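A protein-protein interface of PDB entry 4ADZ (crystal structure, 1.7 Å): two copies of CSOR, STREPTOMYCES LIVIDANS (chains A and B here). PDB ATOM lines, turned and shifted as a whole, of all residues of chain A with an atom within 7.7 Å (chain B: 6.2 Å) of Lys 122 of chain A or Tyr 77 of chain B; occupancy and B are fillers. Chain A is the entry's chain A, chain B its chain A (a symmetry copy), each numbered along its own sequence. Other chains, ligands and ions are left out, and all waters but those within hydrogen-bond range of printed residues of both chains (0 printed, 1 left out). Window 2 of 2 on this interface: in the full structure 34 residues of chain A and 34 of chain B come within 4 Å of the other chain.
Of the 18 printed residues of chain A, 4 touch a printed residue of chain B. Printed residues of chain B that touch a printed residue of chain A: Tyr 77, Cys 78, Ile 79 and Ile 81. Among the printed residues, no Asp or Glu carboxylate lies within 4 Å of a Lys or Arg side-chain nitrogen of the other chain.
The side-chain carboxylate (OE1) of Glu 125 of chain A sits at hydrogen-bond distance from the side-chain hydroxyl (OH) of Tyr 77 of chain B (2.6 Å). ND1 of His 103 of chain A is in hydrogen-bond range of SG of Cys 78 of chain B, at 3.3 Å. The side-chain hydroxyl of Tyr 77 of chain B lies within hydrogen-bond range of the side-chain amino group of Lys 122 of chain A.
No position is printed for both chains. Of the 7 pairs that touch across the chains among the printed residues, none has its exchanged pair printed and touching as well.
Among the printed residues, pairs that only touch across the chains: His 103 of chain A with Tyr 77 of chain B, Leu 99 of chain A with Ile 81 of chain B, Glu 125 of chain A with Ile 79 of chain B and His 103 of chain A with Ile 79 of chain B.
The side-chain sulfur of Cys 107 of chain A lies within hydrogen-bond range of the backbone carbonyl oxygen of His 103 of chain A.
Printed residues of chain B within 4 Å of Leu 99 of chain A: Ile 81 (3.5 Å). Printed residues of chain B within 4 Å of His 103 of chain A: Tyr 77 (3.5 Å), Cys 78 (3.3 Å) and Ile 79 (3.98 Å). Of the printed residues of chain B, Lys 122 of chain A touches Tyr 77 (2.9 Å). Printed residues of chain B within 4 Å of Glu 125 of chain A: Tyr 77 and Ile 79. Of chain A, only His 103, Lys 122 and Glu 125 come within 4 Å of Tyr 77 of chain B. Of the printed residues of chain A, Ile 79 of chain B touches His 103 and Glu 125. The nearest printed residue of chain B that does not touch Lys 122 of chain A is Ile 79 of chain B (6.2 Å). The nearest residue of chain A that does not touch Tyr 77 of chain B is Cys 107 of chain A (6.4 Å). The nearest printed residue of chain A that does not touch Ile 81 of chain B is Glu 125 of chain A (9.0 Å).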
ATOM      1  N   LEU A  99       4.773   5.044   9.494  1.00  0.00           N
ATOM      2  CA  LEU A  99       5.469   3.782   9.080  1.00  0.00           C
ATOM      3  C   LEU A  99       6.634   4.089   8.115  1.00  0.00           C
ATOM      4  O   LEU A  99       7.710   3.500   8.238  1.00  0.00           O
ATOM      5  CB  LEU A  99       4.513   2.791   8.446  1.00  0.00           C
ATOM      6  CG  LEU A  99       3.781   1.775   9.315  1.00  0.00           C
ATOM      7  CD1 LEU A  99       2.994   2.564  10.339  1.00  0.00           C
ATOM      8  CD2 LEU A  99       2.907   0.964   8.357  1.00  0.00           C
ATOM      9  N   HIS A 103      10.584   3.259   8.803  1.00  0.00           N
ATOM     10  CA  HIS A 103      11.339   2.498   7.797  1.00  0.00           C
ATOM     11  C   HIS A 103      12.579   3.199   7.334  1.00  0.00           C
ATOM     12  O   HIS A 103      13.677   2.578   7.261  1.00  0.00           O
ATOM     13  CB  HIS A 103      10.469   2.257   6.606  1.00  0.00           C
ATOM     14  CG  HIS A 103      11.131   1.472   5.514  1.00  0.00           C
ATOM     15  ND1 HIS A 103      11.702   0.250   5.740  1.00  0.00           N
ATOM     16  CD2 HIS A 103      11.210   1.710   4.153  1.00  0.00           C
ATOM     17  CE1 HIS A 103      12.132  -0.245   4.552  1.00  0.00           C
ATOM     18  NE2 HIS A 103      11.881   0.675   3.597  1.00  0.00           N
ATOM     19  N   LEU A 104      12.474   4.491   7.040  1.00  0.00           N
ATOM     20  CA  LEU A 104      13.638   5.268   6.630  1.00  0.00           C
ATOM     21  C   LEU A 104      14.715   5.398   7.730  1.00  0.00           C
ATOM     22  O   LEU A 104      15.918   5.305   7.427  1.00  0.00           O
ATOM     23  CB  LEU A 104      13.236   6.658   6.099  1.00  0.00           C
ATOM     24  CG  LEU A 104      12.448   6.583   4.768  1.00  0.00           C
ATOM     25  CD1 LEU A 104      11.805   7.952   4.412  1.00  0.00           C
ATOM     26  CD2 LEU A 104      13.261   6.036   3.575  1.00  0.00           C
ATOM     27  N   CYS A 107      16.567   2.180   7.687  1.00  0.00           N
ATOM     28  CA  CYS A 107      17.497   2.159   6.539  1.00  0.00           C
ATOM     29  C   CYS A 107      18.760   2.967   6.869  1.00  0.00           C
ATOM     30  O   CYS A 107      19.928   2.515   6.605  1.00  0.00           O
ATOM     31  CB  CYS A 107      16.874   2.727   5.301  1.00  0.00           C
ATOM     32  SG  CYS A 107      15.594   1.668   4.609  1.00  0.00           S
ATOM     33  N   LYS A 114      24.881  -2.437   4.622  1.00  0.00           N
ATOM     34  CA  LYS A 114      24.093  -2.940   3.493  1.00  0.00           C
ATOM     35  C   LYS A 114      24.772  -2.924   2.172  1.00  0.00           C
ATOM     36  O   LYS A 114      24.489  -3.796   1.339  1.00  0.00           O
ATOM     37  CB  LYS A 114      22.766  -2.194   3.409  1.00  0.00           C
ATOM     38  CG  LYS A 114      21.804  -2.488   4.534  1.00  0.00           C
ATOM     39  CD  LYS A 114      21.553  -3.957   4.854  1.00  0.00           C
ATOM     40  CE  LYS A 114      20.717  -4.054   6.131  1.00  0.00           C
ATOM     41  NZ  LYS A 114      20.441  -5.470   6.467  1.00  0.00           N
ATOM     42  N   GLY A 116      25.990  -0.511  -1.415  1.00  0.00           N
ATOM     43  CA  GLY A 116      25.389   0.524  -2.268  1.00  0.00           C
ATOM     44  C   GLY A 116      24.187   0.011  -3.045  1.00  0.00           C
ATOM     45  O   GLY A 116      23.170   0.722  -3.168  1.00  0.00           O
ATOM     46  N   THR A 117      24.276  -1.223  -3.536  1.00  0.00           N
ATOM     47  CA  THR A 117      23.200  -1.802  -4.341  1.00  0.00           C
ATOM     48  C   THR A 117      21.914  -1.946  -3.535  1.00  0.00           C
ATOM     49  O   THR A 117      20.836  -1.538  -3.966  1.00  0.00           O
ATOM     50  CB  THR A 117      23.618  -3.169  -4.915  1.00  0.00           C
ATOM     51  OG1 THR A 117      24.630  -2.922  -5.891  1.00  0.00           O
ATOM     52  CG2 THR A 117      22.406  -3.946  -5.536  1.00  0.00           C
ATOM     53  N   GLU A 118      22.040  -2.513  -2.348  1.00  0.00           N
ATOM     54  CA  GLU A 118      20.881  -2.739  -1.502  1.00  0.00           C
ATOM     55  C   GLU A 118      20.299  -1.395  -1.021  1.00  0.00           C
ATOM     56  O   GLU A 118      19.099  -1.255  -0.958  1.00  0.00           O
ATOM     57  CB  GLU A 118      21.245  -3.671  -0.337  1.00  0.00           C
ATOM     58  CG  GLU A 118      20.031  -4.274   0.373  1.00  0.00           C
ATOM     59  CD  GLU A 118      19.578  -3.488   1.593  1.00  0.00           C
ATOM     60  OE1 GLU A 118      20.022  -2.327   1.702  1.00  0.00           O
ATOM     61  OE2 GLU A 118      18.768  -4.003   2.434  1.00  0.00           O
ATOM     62  N   ILE A 119      21.140  -0.402  -0.724  1.00  0.00           N
ATOM     63  CA  ILE A 119      20.645   0.936  -0.342  1.00  0.00           C
ATOM     64  C   ILE A 119      19.802   1.512  -1.465  1.00  0.00           C
ATOM     65  O   ILE A 119      18.705   1.998  -1.228  1.00  0.00           O
ATOM     66  CB  ILE A 119      21.804   1.932  -0.058  1.00  0.00           C
ATOM     67  CG1 ILE A 119      22.474   1.563   1.303  1.00  0.00           C
ATOM     68  CG2 ILE A 119      21.294   3.396  -0.092  1.00  0.00           C
ATOM     69  CD1 ILE A 119      23.725   2.358   1.697  1.00  0.00           C
ATOM     70  N   ASP A 120      20.344   1.466  -2.676  1.00  0.00           N
ATOM     71  CA  ASP A 120      19.623   1.996  -3.839  1.00  0.00           C
ATOM     72  C   ASP A 120      18.271   1.300  -4.049  1.00  0.00           C
ATOM     73  O   ASP A 120      17.267   1.977  -4.296  1.00  0.00           O
ATOM     74  CB  ASP A 120      20.500   1.884  -5.090  1.00  0.00           C
ATOM     75  CG  ASP A 120      21.702   2.822  -5.044  1.00  0.00           C
ATOM     76  OD1 ASP A 120      21.770   3.710  -4.147  1.00  0.00           O
ATOM     77  OD2 ASP A 120      22.579   2.657  -5.925  1.00  0.00           O
ATOM     78  N   ALA A 121      18.245  -0.027  -3.979  1.00  0.00           N
ATOM     79  CA  ALA A 121      17.027  -0.769  -4.112  1.00  0.00           C
ATOM     80  C   ALA A 121      15.996  -0.402  -3.012  1.00  0.00           C
ATOM     81  O   ALA A 121      14.825  -0.217  -3.328  1.00  0.00           O
ATOM     82  CB  ALA A 121      17.299  -2.292  -4.081  1.00  0.00           C
ATOM     83  N   LYS A 122      16.427  -0.285  -1.741  1.00  0.00           N
ATOM     84  CA  LYS A 122      15.507   0.101  -0.651  1.00  0.00           C
ATOM     85  C   LYS A 122      14.965   1.493  -0.926  1.00  0.00           C
ATOM     86  O   LYS A 122      13.783   1.779  -0.718  1.00  0.00           O
ATOM     87  CB  LYS A 122      16.161   0.096   0.755  1.00  0.00           C
ATOM     88  CG  LYS A 122      16.437  -1.270   1.338  1.00  0.00           C
ATOM     89  CD  LYS A 122      15.124  -2.018   1.672  1.00  0.00           C
ATOM     90  CE  LYS A 122      15.418  -3.461   2.134  1.00  0.00           C
ATOM     91  NZ  LYS A 122      14.211  -4.339   2.097  1.00  0.00           N
ATOM     92  N   VAL A 123      15.834   2.412  -1.373  1.00  0.00           N
ATOM     93  CA  VAL A 123      15.353   3.810  -1.593  1.00  0.00           C
ATOM     94  C   VAL A 123      14.403   3.881  -2.795  1.00  0.00           C
ATOM     95  O   VAL A 123      13.390   4.595  -2.738  1.00  0.00           O
ATOM     96  CB  VAL A 123      16.529   4.786  -1.744  1.00  0.00           C
ATOM     97  CG1 VAL A 123      16.023   6.163  -2.304  1.00  0.00           C
ATOM     98  CG2 VAL A 123      17.181   4.922  -0.373  1.00  0.00           C
ATOM     99  N   GLU A 124      14.684   3.112  -3.853  1.00  0.00           N
ATOM    100  CA  GLU A 124      13.792   3.006  -5.029  1.00  0.00           C
ATOM    101  C   GLU A 124      12.422   2.459  -4.588  1.00  0.00           C
ATOM    102  O   GLU A 124      11.402   3.032  -4.934  1.00  0.00           O
ATOM    103  CB  GLU A 124      14.349   2.130  -6.125  1.00  0.00           C
ATOM    104  CG  GLU A 124      13.388   1.950  -7.302  1.00  0.00           C
ATOM    105  CD  GLU A 124      14.040   1.334  -8.535  1.00  0.00           C
ATOM    106  OE1 GLU A 124      15.264   1.078  -8.522  1.00  0.00           O
ATOM    107  OE2 GLU A 124      13.314   1.123  -9.518  1.00  0.00           O
ATOM    108  N   GLU A 125      12.439   1.427  -3.762  1.00  0.00           N
ATOM    109  CA  GLU A 125      11.200   0.846  -3.278  1.00  0.00           C
ATOM    110  C   GLU A 125      10.421   1.855  -2.437  1.00  0.00           C
ATOM    111  O   GLU A 125       9.195   1.960  -2.596  1.00  0.00           O
ATOM    112  CB  GLU A 125      11.493  -0.380  -2.411  1.00  0.00           C
ATOM    113  CG  GLU A 125      10.246  -1.150  -1.942  1.00  0.00           C
ATOM    114  CD  GLU A 125      10.592  -2.271  -0.966  1.00  0.00           C
ATOM    115  OE1 GLU A 125      11.486  -2.077  -0.052  1.00  0.00           O
ATOM    116  OE2 GLU A 125       9.910  -3.315  -1.107  1.00  0.00           O
ATOM    117  N   ALA A 126      11.068   2.558  -1.535  1.00  0.00           N
ATOM    118  CA  ALA A 126      10.368   3.542  -0.682  1.00  0.00           C
ATOM    119  C   ALA A 126       9.779   4.684  -1.542  1.00  0.00           C
ATOM    120  O   ALA A 126       8.660   5.168  -1.311  1.00  0.00           O
ATOM    121  CB  ALA A 126      11.307   4.092   0.369  1.00  0.00           C
ATOM    122  N   THR A 127      10.534   5.075  -2.565  1.00  0.00           N
ATOM    123  CA  THR A 127      10.116   6.149  -3.416  1.00  0.00           C
ATOM    124  C   THR A 127       8.840   5.703  -4.176  1.00  0.00           C
ATOM    125  O   THR A 127       7.899   6.492  -4.329  1.00  0.00           O
ATOM    126  CB  THR A 127      11.208   6.540  -4.436  1.00  0.00           C
ATOM    127  OG1 THR A 127      12.365   6.995  -3.726  1.00  0.00           O
ATOM    128  CG2 THR A 127      10.659   7.758  -5.387  1.00  0.00           C
ATOM    129  N   LYS A 128       8.802   4.474  -4.654  1.00  0.00           N
ATOM    130  CA  LYS A 128       7.617   3.966  -5.300  1.00  0.00           C
ATOM    131  C   LYS A 128       6.365   3.935  -4.366  1.00  0.00           C
ATOM    132  O   LYS A 128       5.263   4.348  -4.765  1.00  0.00           O
ATOM    133  CB  LYS A 128       7.848   2.604  -5.938  1.00  0.00           C
ATOM    134  CG  LYS A 128       8.720   2.639  -7.189  1.00  0.00           C
ATOM    135  CD  LYS A 128       9.048   1.268  -7.728  1.00  0.00           C
ATOM    136  CE  LYS A 128      10.106   1.412  -8.825  1.00  0.00           C
ATOM    137  NZ  LYS A 128      10.343   0.137  -9.543  1.00  0.00           N
ATOM    138  N   MET B  71      -1.734  -7.265   9.846  1.00  0.00           N
ATOM    139  CA  MET B  71      -0.363  -7.116   9.289  1.00  0.00           C
ATOM    140  C   MET B  71       0.573  -6.514  10.288  1.00  0.00           C
ATOM    141  O   MET B  71       1.743  -6.945  10.415  1.00  0.00           O
ATOM    142  CB  MET B  71      -0.387  -6.261   8.015  1.00  0.00           C
ATOM    143  CG  MET B  71      -1.029  -6.931   6.851  1.00  0.00           C
ATOM    144  SD  MET B  71      -1.431  -5.755   5.490  1.00  0.00           S
ATOM    145  CE  MET B  71      -0.010  -5.951   4.460  1.00  0.00           C
ATOM    146  N   ASP B  75       3.924  -8.283  12.265  1.00  0.00           N
ATOM    147  CA  ASP B  75       5.203  -7.642  11.892  1.00  0.00           C
ATOM    148  C   ASP B  75       5.501  -7.790  10.407  1.00  0.00           C
ATOM    149  O   ASP B  75       6.645  -8.038  10.003  1.00  0.00           O
ATOM    150  CB  ASP B  75       6.397  -8.200  12.709  1.00  0.00           C
ATOM    151  CG  ASP B  75       6.174  -8.127  14.223  1.00  0.00           C
ATOM    152  OD1 ASP B  75       5.456  -7.236  14.730  1.00  0.00           O
ATOM    153  OD2 ASP B  75       6.751  -8.983  14.917  1.00  0.00           O
ATOM    154  N   VAL B  76       4.464  -7.624   9.601  1.00  0.00           N
ATOM    155  CA  VAL B  76       4.568  -7.641   8.141  1.00  0.00           C
ATOM    156  C   VAL B  76       5.437  -6.473   7.676  1.00  0.00           C
ATOM    157  O   VAL B  76       5.426  -5.359   8.255  1.00  0.00           O
ATOM    158  CB  VAL B  76       3.172  -7.684   7.454  1.00  0.00           C
ATOM    159  CG1 VAL B  76       3.213  -7.371   5.939  1.00  0.00           C
ATOM    160  CG2 VAL B  76       2.473  -9.038   7.705  1.00  0.00           C
ATOM    161  N   TYR B  77       6.238  -6.717   6.629  1.00  0.00           N
ATOM    162  CA  TYR B  77       7.136  -5.690   6.119  1.00  0.00           C
ATOM    163  C   TYR B  77       6.367  -4.384   5.829  1.00  0.00           C
ATOM    164  O   TYR B  77       5.280  -4.365   5.248  1.00  0.00           O
ATOM    165  CB  TYR B  77       7.777  -6.193   4.851  1.00  0.00           C
ATOM    166  CG  TYR B  77       8.792  -5.278   4.198  1.00  0.00           C
ATOM    167  CD1 TYR B  77       9.912  -4.846   4.888  1.00  0.00           C
ATOM    168  CD2 TYR B  77       8.685  -4.961   2.855  1.00  0.00           C
ATOM    169  CE1 TYR B  77      10.890  -4.071   4.301  1.00  0.00           C
ATOM    170  CE2 TYR B  77       9.651  -4.176   2.248  1.00  0.00           C
ATOM    171  CZ  TYR B  77      10.720  -3.708   2.984  1.00  0.00           C
ATOM    172  OH  TYR B  77      11.689  -2.940   2.397  1.00  0.00           O
ATOM    173  N   CYS B  78       6.970  -3.306   6.258  1.00  0.00           N
ATOM    174  CA  CYS B  78       6.240  -2.037   6.207  1.00  0.00           C
ATOM    175  C   CYS B  78       5.772  -1.601   4.836  1.00  0.00           C
ATOM    176  O   CYS B  78       4.693  -1.033   4.726  1.00  0.00           O
ATOM    177  CB  CYS B  78       7.017  -0.981   6.881  1.00  0.00           C
ATOM    178  SG  CYS B  78       8.539  -0.727   5.982  1.00  0.00           S
ATOM    179  N   ILE B  79       6.508  -1.872   3.758  1.00  0.00           N
ATOM    180  CA  ILE B  79       6.064  -1.518   2.424  1.00  0.00           C
ATOM    181  C   ILE B  79       4.764  -2.242   2.004  1.00  0.00           C
ATOM    182  O   ILE B  79       3.933  -1.656   1.386  1.00  0.00           O
ATOM    183  CB  ILE B  79       7.178  -1.691   1.351  1.00  0.00           C
ATOM    184  CG1 ILE B  79       8.407  -0.862   1.760  1.00  0.00           C
ATOM    185  CG2 ILE B  79       6.672  -1.354  -0.054  1.00  0.00           C
ATOM    186  CD1 ILE B  79       8.233   0.657   1.736  1.00  0.00           C
ATOM    187  N   ASP B  80       4.618  -3.521   2.361  1.00  0.00           N
ATOM    188  CA  ASP B  80       3.451  -4.297   2.067  1.00  0.00           C
ATOM    189  C   ASP B  80       2.273  -3.645   2.831  1.00  0.00           C
ATOM    190  O   ASP B  80       1.178  -3.549   2.276  1.00  0.00           O
ATOM    191  CB  ASP B  80       3.692  -5.742   2.500  1.00  0.00           C
ATOM    192  CG  ASP B  80       2.700  -6.703   1.981  1.00  0.00           C
ATOM    193  OD1 ASP B  80       2.210  -6.543   0.849  1.00  0.00           O
ATOM    194  OD2 ASP B  80       2.416  -7.718   2.689  1.00  0.00           O
ATOM    195  N   ILE B  81       2.528  -3.168   4.050  1.00  0.00           N
ATOM    196  CA  ILE B  81       1.466  -2.466   4.783  1.00  0.00           C
ATOM    197  C   ILE B  81       1.065  -1.171   4.077  1.00  0.00           C
ATOM    198  O   ILE B  81      -0.148  -0.859   3.947  1.00  0.00           O
ATOM    199  CB  ILE B  81       1.846  -2.211   6.255  1.00  0.00           C
ATOM    200  CG1 ILE B  81       2.096  -3.553   6.983  1.00  0.00           C
ATOM    201  CG2 ILE B  81       0.712  -1.450   6.965  1.00  0.00           C
ATOM    202  CD1 ILE B  81       2.633  -3.449   8.427  1.00  0.00           C
ATOM    203  N   LEU B  82       2.053  -0.386   3.661  1.00  0.00           N
ATOM    204  CA  LEU B  82       1.785   0.835   2.887  1.00  0.00           C
ATOM    205  C   LEU B  82       0.984   0.582   1.652  1.00  0.00           C
ATOM    206  O   LEU B  82       0.015   1.302   1.363  1.00  0.00           O
ATOM    207  CB  LEU B  82       3.062   1.589   2.559  1.00  0.00           C
ATOM    208  CG  LEU B  82       3.864   2.135   3.719  1.00  0.00           C
ATOM    209  CD1 LEU B  82       5.162   2.851   3.239  1.00  0.00           C
ATOM    210  CD2 LEU B  82       3.038   3.078   4.555  1.00  0.00           C
